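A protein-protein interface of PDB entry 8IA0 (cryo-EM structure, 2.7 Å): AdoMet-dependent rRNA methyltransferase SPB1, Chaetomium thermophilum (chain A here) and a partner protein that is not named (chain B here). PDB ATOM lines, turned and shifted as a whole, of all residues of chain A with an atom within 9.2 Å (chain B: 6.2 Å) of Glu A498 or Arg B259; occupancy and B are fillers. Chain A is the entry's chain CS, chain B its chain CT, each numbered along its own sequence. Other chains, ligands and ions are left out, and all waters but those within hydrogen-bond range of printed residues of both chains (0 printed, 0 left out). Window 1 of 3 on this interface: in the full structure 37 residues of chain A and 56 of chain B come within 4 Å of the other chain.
The side-chain carboxylate (OE1) of Glu A498 lies within salt-bridge range of the guanidinium group (NH2) of Arg B183, 3.1 Å away. OE1 of Glu A498 lies within salt-bridge range of NH2 of Arg B259, 2.9 Å away. OE2 of Glu A498 sits close to ND2 of Asn B297 (3.5 Å). The backbone NH (N) of Phe B258 lies within hydrogen-bond range of the side-chain carboxylate (OD1) of Asp A501 (3.4 Å). The indole nitrogen (NE1) of Trp A504 sits close to the side-chain amide nitrogen (ND2) of Asn B257. The backbone carbonyl oxygen (O) of Val A499 lies close to the guanidinium group (NH1) of Arg B183, 2.3 Å away.
N of Asp A501 sits close to OE2 of Glu A503 (3.4 Å). The guanidinium group (NE) of Arg B183 sits at hydrogen-bond distance from the backbone carbonyl oxygen (O) of His B255, at 2.8 Å. The backbone carbonyl oxygen (O) of Phe B256 sits at hydrogen-bond distance from the guanidinium group (NH2) of Arg B183 (3.1 Å). The guanidinium group of Arg B259 sits close to the backbone carbonyl oxygen of Pro B254 (3.5 Å). The side-chain carboxylate (OE1) of Glu B301 is in salt-bridge range of the guanidinium group (NH2) of Arg B259.
Of chain B, only Arg B183 (3.1 Å), Arg B259 (2.9 Å) and Asn B297 (3.1 Å) come within 4 Å of Glu A498. Of the printed residues of chain B, Val A499 touches Arg B183. Of the printed residues of chain B, Asp A501 touches Phe B258. Printed residues of chain A within 4 Å of Asn B257: Trp A504. Of the printed residues of chain A, Arg B259 touches Glu A498. Gly B260 touches none of the printed residues of chain A. Leu B262 touches none of the printed residues of chain A. No residue of chain A comes within 4 Å of Ala B298. Leu B305 touches none of the printed residues of chain A. The nearest printed residue of chain A that does not touch Asn B297 is Arg A496 (5.1 Å).
Hydrophobic or aromatic side chains of chain A that line the printed part of chain B: Val A499 and Trp A504. Of the 22 printed residues of chain B, 5 touch a printed residue of chain A. Printed residues of chain B that touch a printed residue of chain A: Arg B183, Asn B257, Phe B258, Arg B259 and Asn B297. Hydrophobic or aromatic side chains of chain B that line the printed part of chain A: Phe B258. Among the printed residues, 6 pairs touch across the chains.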
ATOM      1  N   ALA A 492      20.074  34.997  19.184  1.00  0.00           N
ATOM      2  CA  ALA A 492      19.645  35.045  20.576  1.00  0.00           C
ATOM      3  C   ALA A 492      18.200  34.588  20.723  1.00  0.00           C
ATOM      4  O   ALA A 492      17.870  33.836  21.648  1.00  0.00           O
ATOM      5  CB  ALA A 492      19.820  36.457  21.132  1.00  0.00           C
ATOM      6  N   LYS A 493      17.325  35.034  19.821  1.00  0.00           N
ATOM      7  CA  LYS A 493      15.929  34.614  19.870  1.00  0.00           C
ATOM      8  C   LYS A 493      15.795  33.114  19.644  1.00  0.00           C
ATOM      9  O   LYS A 493      14.994  32.447  20.309  1.00  0.00           O
ATOM     10  CB  LYS A 493      15.113  35.390  18.838  1.00  0.00           C
ATOM     11  CG  LYS A 493      14.331  36.555  19.415  1.00  0.00           C
ATOM     12  CD  LYS A 493      13.113  36.874  18.567  1.00  0.00           C
ATOM     13  CE  LYS A 493      13.494  37.694  17.345  1.00  0.00           C
ATOM     14  NZ  LYS A 493      14.387  38.831  17.698  1.00  0.00           N
ATOM     15  N   ARG A 494      16.571  32.566  18.708  1.00  0.00           N
ATOM     16  CA  ARG A 494      16.530  31.130  18.460  1.00  0.00           C
ATOM     17  C   ARG A 494      17.096  30.348  19.639  1.00  0.00           C
ATOM     18  O   ARG A 494      16.613  29.254  19.955  1.00  0.00           O
ATOM     19  CB  ARG A 494      17.295  30.798  17.180  1.00  0.00           C
ATOM     20  CG  ARG A 494      17.198  29.344  16.756  1.00  0.00           C
ATOM     21  CD  ARG A 494      18.086  29.061  15.558  1.00  0.00           C
ATOM     22  NE  ARG A 494      19.264  29.919  15.538  1.00  0.00           N
ATOM     23  CZ  ARG A 494      20.481  29.529  15.895  1.00  0.00           C
ATOM     24  NH1 ARG A 494      20.718  28.295  16.309  1.00  0.00           N
ATOM     25  NH2 ARG A 494      21.485  30.399  15.835  1.00  0.00           N
ATOM     26  N   ALA A 495      18.124  30.889  20.298  1.00  0.00           N
ATOM     27  CA  ALA A 495      18.715  30.202  21.441  1.00  0.00           C
ATOM     28  C   ALA A 495      17.720  30.076  22.587  1.00  0.00           C
ATOM     29  O   ALA A 495      17.647  29.032  23.245  1.00  0.00           O
ATOM     30  CB  ALA A 495      19.974  30.934  21.901  1.00  0.00           C
ATOM     31  N   ARG A 496      16.945  31.126  22.842  1.00  0.00           N
ATOM     32  CA  ARG A 496      15.952  31.111  23.907  1.00  0.00           C
ATOM     33  C   ARG A 496      14.614  30.536  23.470  1.00  0.00           C
ATOM     34  O   ARG A 496      13.739  30.336  24.317  1.00  0.00           O
ATOM     35  CB  ARG A 496      15.744  32.524  24.457  1.00  0.00           C
ATOM     36  CG  ARG A 496      16.896  33.020  25.306  1.00  0.00           C
ATOM     37  CD  ARG A 496      16.806  34.515  25.554  1.00  0.00           C
ATOM     38  NE  ARG A 496      16.747  34.844  26.975  1.00  0.00           N
ATOM     39  CZ  ARG A 496      17.687  34.558  27.867  1.00  0.00           C
ATOM     40  NH1 ARG A 496      18.826  33.979  27.516  1.00  0.00           N
ATOM     41  NH2 ARG A 496      17.488  34.876  29.143  1.00  0.00           N
ATOM     42  N   GLN A 497      14.430  30.272  22.180  1.00  0.00           N
ATOM     43  CA  GLN A 497      13.176  29.702  21.708  1.00  0.00           C
ATOM     44  C   GLN A 497      13.006  28.287  22.244  1.00  0.00           C
ATOM     45  O   GLN A 497      13.945  27.488  22.245  1.00  0.00           O
ATOM     46  CB  GLN A 497      13.135  29.700  20.181  1.00  0.00           C
ATOM     47  CG  GLN A 497      11.895  29.059  19.591  1.00  0.00           C
ATOM     48  CD  GLN A 497      12.018  28.820  18.100  1.00  0.00           C
ATOM     49  OE1 GLN A 497      12.748  29.526  17.405  1.00  0.00           O
ATOM     50  NE2 GLN A 497      11.304  27.819  17.601  1.00  0.00           N
ATOM     51  N   GLU A 498      11.799  27.982  22.704  1.00  0.00           N
ATOM     52  CA  GLU A 498      11.493  26.696  23.307  1.00  0.00           C
ATOM     53  C   GLU A 498      11.012  25.710  22.249  1.00  0.00           C
ATOM     54  O   GLU A 498      10.558  26.088  21.167  1.00  0.00           O
ATOM     55  CB  GLU A 498      10.434  26.850  24.399  1.00  0.00           C
ATOM     56  CG  GLU A 498      10.475  25.766  25.463  1.00  0.00           C
ATOM     57  CD  GLU A 498       9.827  26.203  26.758  1.00  0.00           C
ATOM     58  OE1 GLU A 498       9.575  25.338  27.623  1.00  0.00           O
ATOM     59  OE2 GLU A 498       9.568  27.413  26.909  1.00  0.00           O
ATOM     60  N   VAL A 499      11.123  24.428  22.581  1.00  0.00           N
ATOM     61  CA  VAL A 499      10.695  23.342  21.710  1.00  0.00           C
ATOM     62  C   VAL A 499       9.284  22.940  22.113  1.00  0.00           C
ATOM     63  O   VAL A 499       9.044  22.571  23.269  1.00  0.00           O
ATOM     64  CB  VAL A 499      11.660  22.148  21.803  1.00  0.00           C
ATOM     65  CG1 VAL A 499      11.213  21.022  20.890  1.00  0.00           C
ATOM     66  CG2 VAL A 499      13.075  22.588  21.476  1.00  0.00           C
ATOM     67  N   ASP A 500       8.355  23.004  21.166  1.00  0.00           N
ATOM     68  CA  ASP A 500       6.961  22.720  21.463  1.00  0.00           C
ATOM     69  C   ASP A 500       6.754  21.225  21.704  1.00  0.00           C
ATOM     70  O   ASP A 500       7.690  20.423  21.677  1.00  0.00           O
ATOM     71  CB  ASP A 500       6.065  23.212  20.328  1.00  0.00           C
ATOM     72  CG  ASP A 500       4.653  23.525  20.790  1.00  0.00           C
ATOM     73  OD1 ASP A 500       4.413  23.514  22.016  1.00  0.00           O
ATOM     74  OD2 ASP A 500       3.786  23.781  19.929  1.00  0.00           O
ATOM     75  N   ASP A 501       5.500  20.854  21.951  1.00  0.00           N
ATOM     76  CA  ASP A 501       5.147  19.458  22.169  1.00  0.00           C
ATOM     77  C   ASP A 501       4.471  18.829  20.960  1.00  0.00           C
ATOM     78  O   ASP A 501       4.341  17.602  20.903  1.00  0.00           O
ATOM     79  CB  ASP A 501       4.226  19.329  23.385  1.00  0.00           C
ATOM     80  CG  ASP A 501       4.977  19.422  24.697  1.00  0.00           C
ATOM     81  OD1 ASP A 501       6.175  19.068  24.726  1.00  0.00           O
ATOM     82  OD2 ASP A 501       4.371  19.852  25.701  1.00  0.00           O
ATOM     83  N   GLU A 503       5.430  18.793  17.709  1.00  0.00           N
ATOM     84  CA  GLU A 503       6.332  18.041  16.847  1.00  0.00           C
ATOM     85  C   GLU A 503       6.770  16.737  17.498  1.00  0.00           C
ATOM     86  O   GLU A 503       7.207  15.815  16.797  1.00  0.00           O
ATOM     87  CB  GLU A 503       7.554  18.883  16.458  1.00  0.00           C
ATOM     88  CG  GLU A 503       8.480  19.383  17.581  1.00  0.00           C
ATOM     89  CD  GLU A 503       7.829  20.319  18.596  1.00  0.00           C
ATOM     90  OE1 GLU A 503       8.565  21.156  19.156  1.00  0.00           O
ATOM     91  OE2 GLU A 503       6.609  20.238  18.844  1.00  0.00           O
ATOM     92  N   TRP A 504       6.663  16.638  18.821  1.00  0.00           N
ATOM     93  CA  TRP A 504       6.877  15.374  19.508  1.00  0.00           C
ATOM     94  C   TRP A 504       5.655  14.472  19.475  1.00  0.00           C
ATOM     95  O   TRP A 504       5.738  13.329  19.936  1.00  0.00           O
ATOM     96  CB  TRP A 504       7.285  15.620  20.960  1.00  0.00           C
ATOM     97  CG  TRP A 504       8.747  15.816  21.136  1.00  0.00           C
ATOM     98  CD1 TRP A 504       9.378  16.950  21.545  1.00  0.00           C
ATOM     99  CD2 TRP A 504       9.772  14.849  20.893  1.00  0.00           C
ATOM    100  NE1 TRP A 504      10.735  16.749  21.580  1.00  0.00           N
ATOM    101  CE2 TRP A 504      11.002  15.465  21.184  1.00  0.00           C
ATOM    102  CE3 TRP A 504       9.769  13.520  20.461  1.00  0.00           C
ATOM    103  CZ2 TRP A 504      12.214  14.800  21.055  1.00  0.00           C
ATOM    104  CZ3 TRP A 504      10.973  12.865  20.335  1.00  0.00           C
ATOM    105  CH2 TRP A 504      12.178  13.504  20.631  1.00  0.00           C
ATOM    106  N   ARG B 183      15.899  21.245  26.156  1.00  0.00           N
ATOM    107  CA  ARG B 183      15.035  20.331  25.433  1.00  0.00           C
ATOM    108  C   ARG B 183      15.759  19.798  24.200  1.00  0.00           C
ATOM    109  O   ARG B 183      16.727  20.390  23.714  1.00  0.00           O
ATOM    110  CB  ARG B 183      13.736  21.028  25.030  1.00  0.00           C
ATOM    111  CG  ARG B 183      12.856  21.419  26.205  1.00  0.00           C
ATOM    112  CD  ARG B 183      11.521  21.976  25.743  1.00  0.00           C
ATOM    113  NE  ARG B 183      10.578  22.107  26.846  1.00  0.00           N
ATOM    114  CZ  ARG B 183       9.290  22.381  26.701  1.00  0.00           C
ATOM    115  NH1 ARG B 183       8.751  22.558  25.508  1.00  0.00           N
ATOM    116  NH2 ARG B 183       8.521  22.478  27.782  1.00  0.00           N
ATOM    117  N   TYR B 214      10.605   9.248  29.378  1.00  0.00           N
ATOM    118  CA  TYR B 214       9.948  10.304  30.141  1.00  0.00           C
ATOM    119  C   TYR B 214       8.483  10.437  29.751  1.00  0.00           C
ATOM    120  O   TYR B 214       7.621  10.649  30.612  1.00  0.00           O
ATOM    121  CB  TYR B 214      10.674  11.632  29.943  1.00  0.00           C
ATOM    122  CG  TYR B 214      10.334  12.659  30.997  1.00  0.00           C
ATOM    123  CD1 TYR B 214      10.239  12.301  32.333  1.00  0.00           C
ATOM    124  CD2 TYR B 214      10.101  13.982  30.656  1.00  0.00           C
ATOM    125  CE1 TYR B 214       9.926  13.234  33.301  1.00  0.00           C
ATOM    126  CE2 TYR B 214       9.787  14.921  31.619  1.00  0.00           C
ATOM    127  CZ  TYR B 214       9.702  14.540  32.938  1.00  0.00           C
ATOM    128  OH  TYR B 214       9.389  15.472  33.901  1.00  0.00           O
ATOM    129  N   LEU B 218       5.461   9.773  32.509  1.00  0.00           N
ATOM    130  CA  LEU B 218       4.426  10.736  32.865  1.00  0.00           C
ATOM    131  C   LEU B 218       3.036  10.154  32.653  1.00  0.00           C
ATOM    132  O   LEU B 218       2.105  10.470  33.404  1.00  0.00           O
ATOM    133  CB  LEU B 218       4.607  12.020  32.060  1.00  0.00           C
ATOM    134  CG  LEU B 218       5.833  12.845  32.445  1.00  0.00           C
ATOM    135  CD1 LEU B 218       5.790  14.219  31.796  1.00  0.00           C
ATOM    136  CD2 LEU B 218       5.951  12.957  33.953  1.00  0.00           C
ATOM    137  N   VAL B 250       8.212  18.787  39.006  1.00  0.00           N
ATOM    138  CA  VAL B 250       7.828  20.146  38.630  1.00  0.00           C
ATOM    139  C   VAL B 250       8.866  21.147  39.120  1.00  0.00           C
ATOM    140  O   VAL B 250       9.286  22.046  38.384  1.00  0.00           O
ATOM    141  CB  VAL B 250       6.425  20.476  39.172  1.00  0.00           C
ATOM    142  CG1 VAL B 250       6.256  21.973  39.350  1.00  0.00           C
ATOM    143  CG2 VAL B 250       5.354  19.928  38.247  1.00  0.00           C
ATOM    144  N   VAL B 253      12.674  19.821  37.248  1.00  0.00           N
ATOM    145  CA  VAL B 253      12.890  19.892  35.804  1.00  0.00           C
ATOM    146  C   VAL B 253      11.678  20.509  35.115  1.00  0.00           C
ATOM    147  O   VAL B 253      10.934  19.803  34.421  1.00  0.00           O
ATOM    148  CB  VAL B 253      13.212  18.504  35.229  1.00  0.00           C
ATOM    149  CG1 VAL B 253      14.674  18.172  35.465  1.00  0.00           C
ATOM    150  CG2 VAL B 253      12.333  17.446  35.868  1.00  0.00           C
ATOM    151  N   PRO B 254      11.442  21.813  35.265  1.00  0.00           N
ATOM    152  CA  PRO B 254      10.322  22.441  34.553  1.00  0.00           C
ATOM    153  C   PRO B 254      10.638  22.681  33.087  1.00  0.00           C
ATOM    154  O   PRO B 254       9.763  22.568  32.224  1.00  0.00           O
ATOM    155  CB  PRO B 254      10.120  23.767  35.303  1.00  0.00           C
ATOM    156  CG  PRO B 254      11.114  23.766  36.442  1.00  0.00           C
ATOM    157  CD  PRO B 254      12.175  22.784  36.089  1.00  0.00           C
ATOM    158  N   HIS B 255      11.898  23.010  32.800  1.00  0.00           N
ATOM    159  CA  HIS B 255      12.310  23.384  31.454  1.00  0.00           C
ATOM    160  C   HIS B 255      12.156  22.255  30.444  1.00  0.00           C
ATOM    161  O   HIS B 255      11.987  22.530  29.251  1.00  0.00           O
ATOM    162  CB  HIS B 255      13.765  23.843  31.473  1.00  0.00           C
ATOM    163  CG  HIS B 255      14.720  22.772  31.897  1.00  0.00           C
ATOM    164  ND1 HIS B 255      14.929  22.443  33.218  1.00  0.00           N
ATOM    165  CD2 HIS B 255      15.510  21.945  31.174  1.00  0.00           C
ATOM    166  CE1 HIS B 255      15.812  21.465  33.291  1.00  0.00           C
ATOM    167  NE2 HIS B 255      16.182  21.144  32.065  1.00  0.00           N
ATOM    168  N   PHE B 256      12.208  21.003  30.885  1.00  0.00           N
ATOM    169  CA  PHE B 256      12.270  19.874  29.970  1.00  0.00           C
ATOM    170  C   PHE B 256      10.935  19.695  29.245  1.00  0.00           C
ATOM    171  O   PHE B 256       9.950  20.391  29.504  1.00  0.00           O
ATOM    172  CB  PHE B 256      12.666  18.609  30.727  1.00  0.00           C
ATOM    173  CG  PHE B 256      13.238  17.535  29.852  1.00  0.00           C
ATOM    174  CD1 PHE B 256      14.199  17.837  28.904  1.00  0.00           C
ATOM    175  CD2 PHE B 256      12.812  16.224  29.971  1.00  0.00           C
ATOM    176  CE1 PHE B 256      14.724  16.854  28.095  1.00  0.00           C
ATOM    177  CE2 PHE B 256      13.336  15.237  29.164  1.00  0.00           C
ATOM    178  CZ  PHE B 256      14.293  15.553  28.225  1.00  0.00           C
ATOM    179  N   ASN B 257      10.908  18.737  28.321  1.00  0.00           N
ATOM    180  CA  ASN B 257       9.741  18.500  27.489  1.00  0.00           C
ATOM    181  C   ASN B 257       8.578  17.965  28.321  1.00  0.00           C
ATOM    182  O   ASN B 257       8.731  17.554  29.475  1.00  0.00           O
ATOM    183  CB  ASN B 257      10.069  17.514  26.368  1.00  0.00           C
ATOM    184  CG  ASN B 257      11.339  17.869  25.632  1.00  0.00           C
ATOM    185  OD1 ASN B 257      12.422  17.897  26.214  1.00  0.00           O
ATOM    186  ND2 ASN B 257      11.215  18.143  24.339  1.00  0.00           N
ATOM    187  N   PHE B 258       7.396  17.975  27.703  1.00  0.00           N
ATOM    188  CA  PHE B 258       6.163  17.454  28.288  1.00  0.00           C
ATOM    189  C   PHE B 258       5.831  18.108  29.623  1.00  0.00           C
ATOM    190  O   PHE B 258       5.345  17.441  30.542  1.00  0.00           O
ATOM    191  CB  PHE B 258       6.228  15.931  28.440  1.00  0.00           C
ATOM    192  CG  PHE B 258       6.834  15.237  27.257  1.00  0.00           C
ATOM    193  CD1 PHE B 258       6.331  15.443  25.987  1.00  0.00           C
ATOM    194  CD2 PHE B 258       7.912  14.385  27.416  1.00  0.00           C
ATOM    195  CE1 PHE B 258       6.887  14.810  24.897  1.00  0.00           C
ATOM    196  CE2 PHE B 258       8.472  13.748  26.329  1.00  0.00           C
ATOM    197  CZ  PHE B 258       7.959  13.960  25.069  1.00  0.00           C
ATOM    198  N   ARG B 259       6.095  19.410  29.741  1.00  0.00           N
ATOM    199  CA  ARG B 259       5.735  20.140  30.950  1.00  0.00           C
ATOM    200  C   ARG B 259       4.228  20.180  31.149  1.00  0.00           C
ATOM    201  O   ARG B 259       3.750  20.144  32.289  1.00  0.00           O
ATOM    202  CB  ARG B 259       6.306  21.556  30.883  1.00  0.00           C
ATOM    203  CG  ARG B 259       6.080  22.390  32.126  1.00  0.00           C
ATOM    204  CD  ARG B 259       6.815  23.714  32.018  1.00  0.00           C
ATOM    205  NE  ARG B 259       6.533  24.391  30.759  1.00  0.00           N
ATOM    206  CZ  ARG B 259       7.388  25.183  30.128  1.00  0.00           C
ATOM    207  NH1 ARG B 259       8.601  25.408  30.603  1.00  0.00           N
ATOM    208  NH2 ARG B 259       7.018  25.762  28.991  1.00  0.00           N
ATOM    209  N   GLY B 260       3.464  20.257  30.059  1.00  0.00           N
ATOM    210  CA  GLY B 260       2.016  20.290  30.184  1.00  0.00           C
ATOM    211  C   GLY B 260       1.456  19.013  30.776  1.00  0.00           C
ATOM    212  O   GLY B 260       0.567  19.048  31.629  1.00  0.00           O
ATOM    213  N   ASP B 261       1.973  17.866  30.332  1.00  0.00           N
ATOM    214  CA  ASP B 261       1.530  16.592  30.888  1.00  0.00           C
ATOM    215  C   ASP B 261       1.834  16.511  32.377  1.00  0.00           C
ATOM    216  O   ASP B 261       1.056  15.940  33.148  1.00  0.00           O
ATOM    217  CB  ASP B 261       2.188  15.436  30.139  1.00  0.00           C
ATOM    218  CG  ASP B 261       1.957  15.505  28.643  1.00  0.00           C
ATOM    219  OD1 ASP B 261       1.160  16.360  28.203  1.00  0.00           O
ATOM    220  OD2 ASP B 261       2.571  14.704  27.907  1.00  0.00           O
ATOM    221  N   LEU B 262       2.964  17.077  32.797  1.00  0.00           N
ATOM    222  CA  LEU B 262       3.285  17.129  34.218  1.00  0.00           C
ATOM    223  C   LEU B 262       2.357  18.086  34.955  1.00  0.00           C
ATOM    224  O   LEU B 262       1.859  17.774  36.043  1.00  0.00           O
ATOM    225  CB  LEU B 262       4.746  17.540  34.403  1.00  0.00           C
ATOM    226  CG  LEU B 262       5.384  17.251  35.759  1.00  0.00           C
ATOM    227  CD1 LEU B 262       5.258  15.783  36.110  1.00  0.00           C
ATOM    228  CD2 LEU B 262       6.840  17.680  35.749  1.00  0.00           C
ATOM    229  N   LEU B 263       2.109  19.261  34.374  1.00  0.00           N
ATOM    230  CA  LEU B 263       1.267  20.251  35.034  1.00  0.00           C
ATOM    231  C   LEU B 263      -0.203  19.856  35.006  1.00  0.00           C
ATOM    232  O   LEU B 263      -0.971  20.282  35.875  1.00  0.00           O
ATOM    233  CB  LEU B 263       1.462  21.620  34.388  1.00  0.00           C
ATOM    234  CG  LEU B 263       2.779  22.326  34.707  1.00  0.00           C
ATOM    235  CD1 LEU B 263       2.890  23.628  33.935  1.00  0.00           C
ATOM    236  CD2 LEU B 263       2.902  22.571  36.198  1.00  0.00           C
ATOM    237  N   ARG B 264      -0.616  19.055  34.022  1.00  0.00           N
ATOM    238  CA  ARG B 264      -2.012  18.636  33.958  1.00  0.00           C
ATOM    239  C   ARG B 264      -2.363  17.698  35.105  1.00  0.00           C
ATOM    240  O   ARG B 264      -3.514  17.664  35.554  1.00  0.00           O
ATOM    241  CB  ARG B 264      -2.305  17.980  32.611  1.00  0.00           C
ATOM    242  CG  ARG B 264      -2.570  18.974  31.499  1.00  0.00           C
ATOM    243  CD  ARG B 264      -2.869  18.276  30.193  1.00  0.00           C
ATOM    244  NE  ARG B 264      -2.562  19.124  29.050  1.00  0.00           N
ATOM    245  CZ  ARG B 264      -3.378  20.045  28.560  1.00  0.00           C
ATOM    246  NH1 ARG B 264      -4.568  20.268  29.092  1.00  0.00           N
ATOM    247  NH2 ARG B 264      -2.991  20.764  27.511  1.00  0.00           N
ATOM    248  N   LEU B 289       6.787  26.986  42.070  1.00  0.00           N
ATOM    249  CA  LEU B 289       7.133  27.185  40.667  1.00  0.00           C
ATOM    250  C   LEU B 289       6.889  28.623  40.231  1.00  0.00           C
ATOM    251  O   LEU B 289       7.698  29.201  39.495  1.00  0.00           O
ATOM    252  CB  LEU B 289       6.342  26.218  39.788  1.00  0.00           C
ATOM    253  CG  LEU B 289       6.517  26.391  38.280  1.00  0.00           C
ATOM    254  CD1 LEU B 289       7.840  25.806  37.828  1.00  0.00           C
ATOM    255  CD2 LEU B 289       5.367  25.745  37.534  1.00  0.00           C
ATOM    256  N   ASN B 297       8.276  31.017  30.967  1.00  0.00           N
ATOM    257  CA  ASN B 297       7.589  30.042  30.125  1.00  0.00           C
ATOM    258  C   ASN B 297       6.812  29.036  30.964  1.00  0.00           C
ATOM    259  O   ASN B 297       5.671  28.689  30.636  1.00  0.00           O
ATOM    260  CB  ASN B 297       8.594  29.332  29.222  1.00  0.00           C
ATOM    261  CG  ASN B 297       9.209  30.259  28.198  1.00  0.00           C
ATOM    262  OD1 ASN B 297       8.517  30.788  27.329  1.00  0.00           O
ATOM    263  ND2 ASN B 297      10.518  30.460  28.292  1.00  0.00           N
ATOM    264  N   ALA B 298       7.416  28.547  32.048  1.00  0.00           N
ATOM    265  CA  ALA B 298       6.718  27.605  32.915  1.00  0.00           C
ATOM    266  C   ALA B 298       5.518  28.260  33.583  1.00  0.00           C
ATOM    267  O   ALA B 298       4.456  27.642  33.715  1.00  0.00           O
ATOM    268  CB  ALA B 298       7.678  27.042  33.963  1.00  0.00           C
ATOM    269  N   SER B 299       5.670  29.514  34.014  1.00  0.00           N
ATOM    270  CA  SER B 299       4.563  30.219  34.649  1.00  0.00           C
ATOM    271  C   SER B 299       3.405  30.422  33.682  1.00  0.00           C
ATOM    272  O   SER B 299       2.239  30.248  34.054  1.00  0.00           O
ATOM    273  CB  SER B 299       5.044  31.562  35.195  1.00  0.00           C
ATOM    274  OG  SER B 299       5.674  31.403  36.453  1.00  0.00           O
ATOM    275  N   GLU B 301       2.486  28.692  31.025  1.00  0.00           N
ATOM    276  CA  GLU B 301       1.770  27.468  30.687  1.00  0.00           C
ATOM    277  C   GLU B 301       0.887  27.011  31.840  1.00  0.00           C
ATOM    278  O   GLU B 301      -0.207  26.479  31.620  1.00  0.00           O
ATOM    279  CB  GLU B 301       2.769  26.383  30.289  1.00  0.00           C
ATOM    280  CG  GLU B 301       2.164  25.015  30.056  1.00  0.00           C
ATOM    281  CD  GLU B 301       2.896  24.249  28.974  1.00  0.00           C
ATOM    282  OE1 GLU B 301       3.695  24.871  28.243  1.00  0.00           O
ATOM    283  OE2 GLU B 301       2.670  23.030  28.847  1.00  0.00           O
ATOM    284  N   LEU B 305      -3.359  26.925  32.028  1.00  0.00           N
ATOM    285  CA  LEU B 305      -4.088  25.757  32.510  1.00  0.00           C
ATOM    286  C   LEU B 305      -5.044  26.126  33.635  1.00  0.00           C
ATOM    287  O   LEU B 305      -6.200  25.689  33.647  1.00  0.00           O
ATOM    288  CB  LEU B 305      -3.106  24.684  32.975  1.00  0.00           C
ATOM    289  CG  LEU B 305      -2.440  23.856  31.877  1.00  0.00           C
ATOM    290  CD1 LEU B 305      -1.613  22.737  32.480  1.00  0.00           C
ATOM    291  CD2 LEU B 305      -3.485  23.300  30.929  1.00  0.00           C
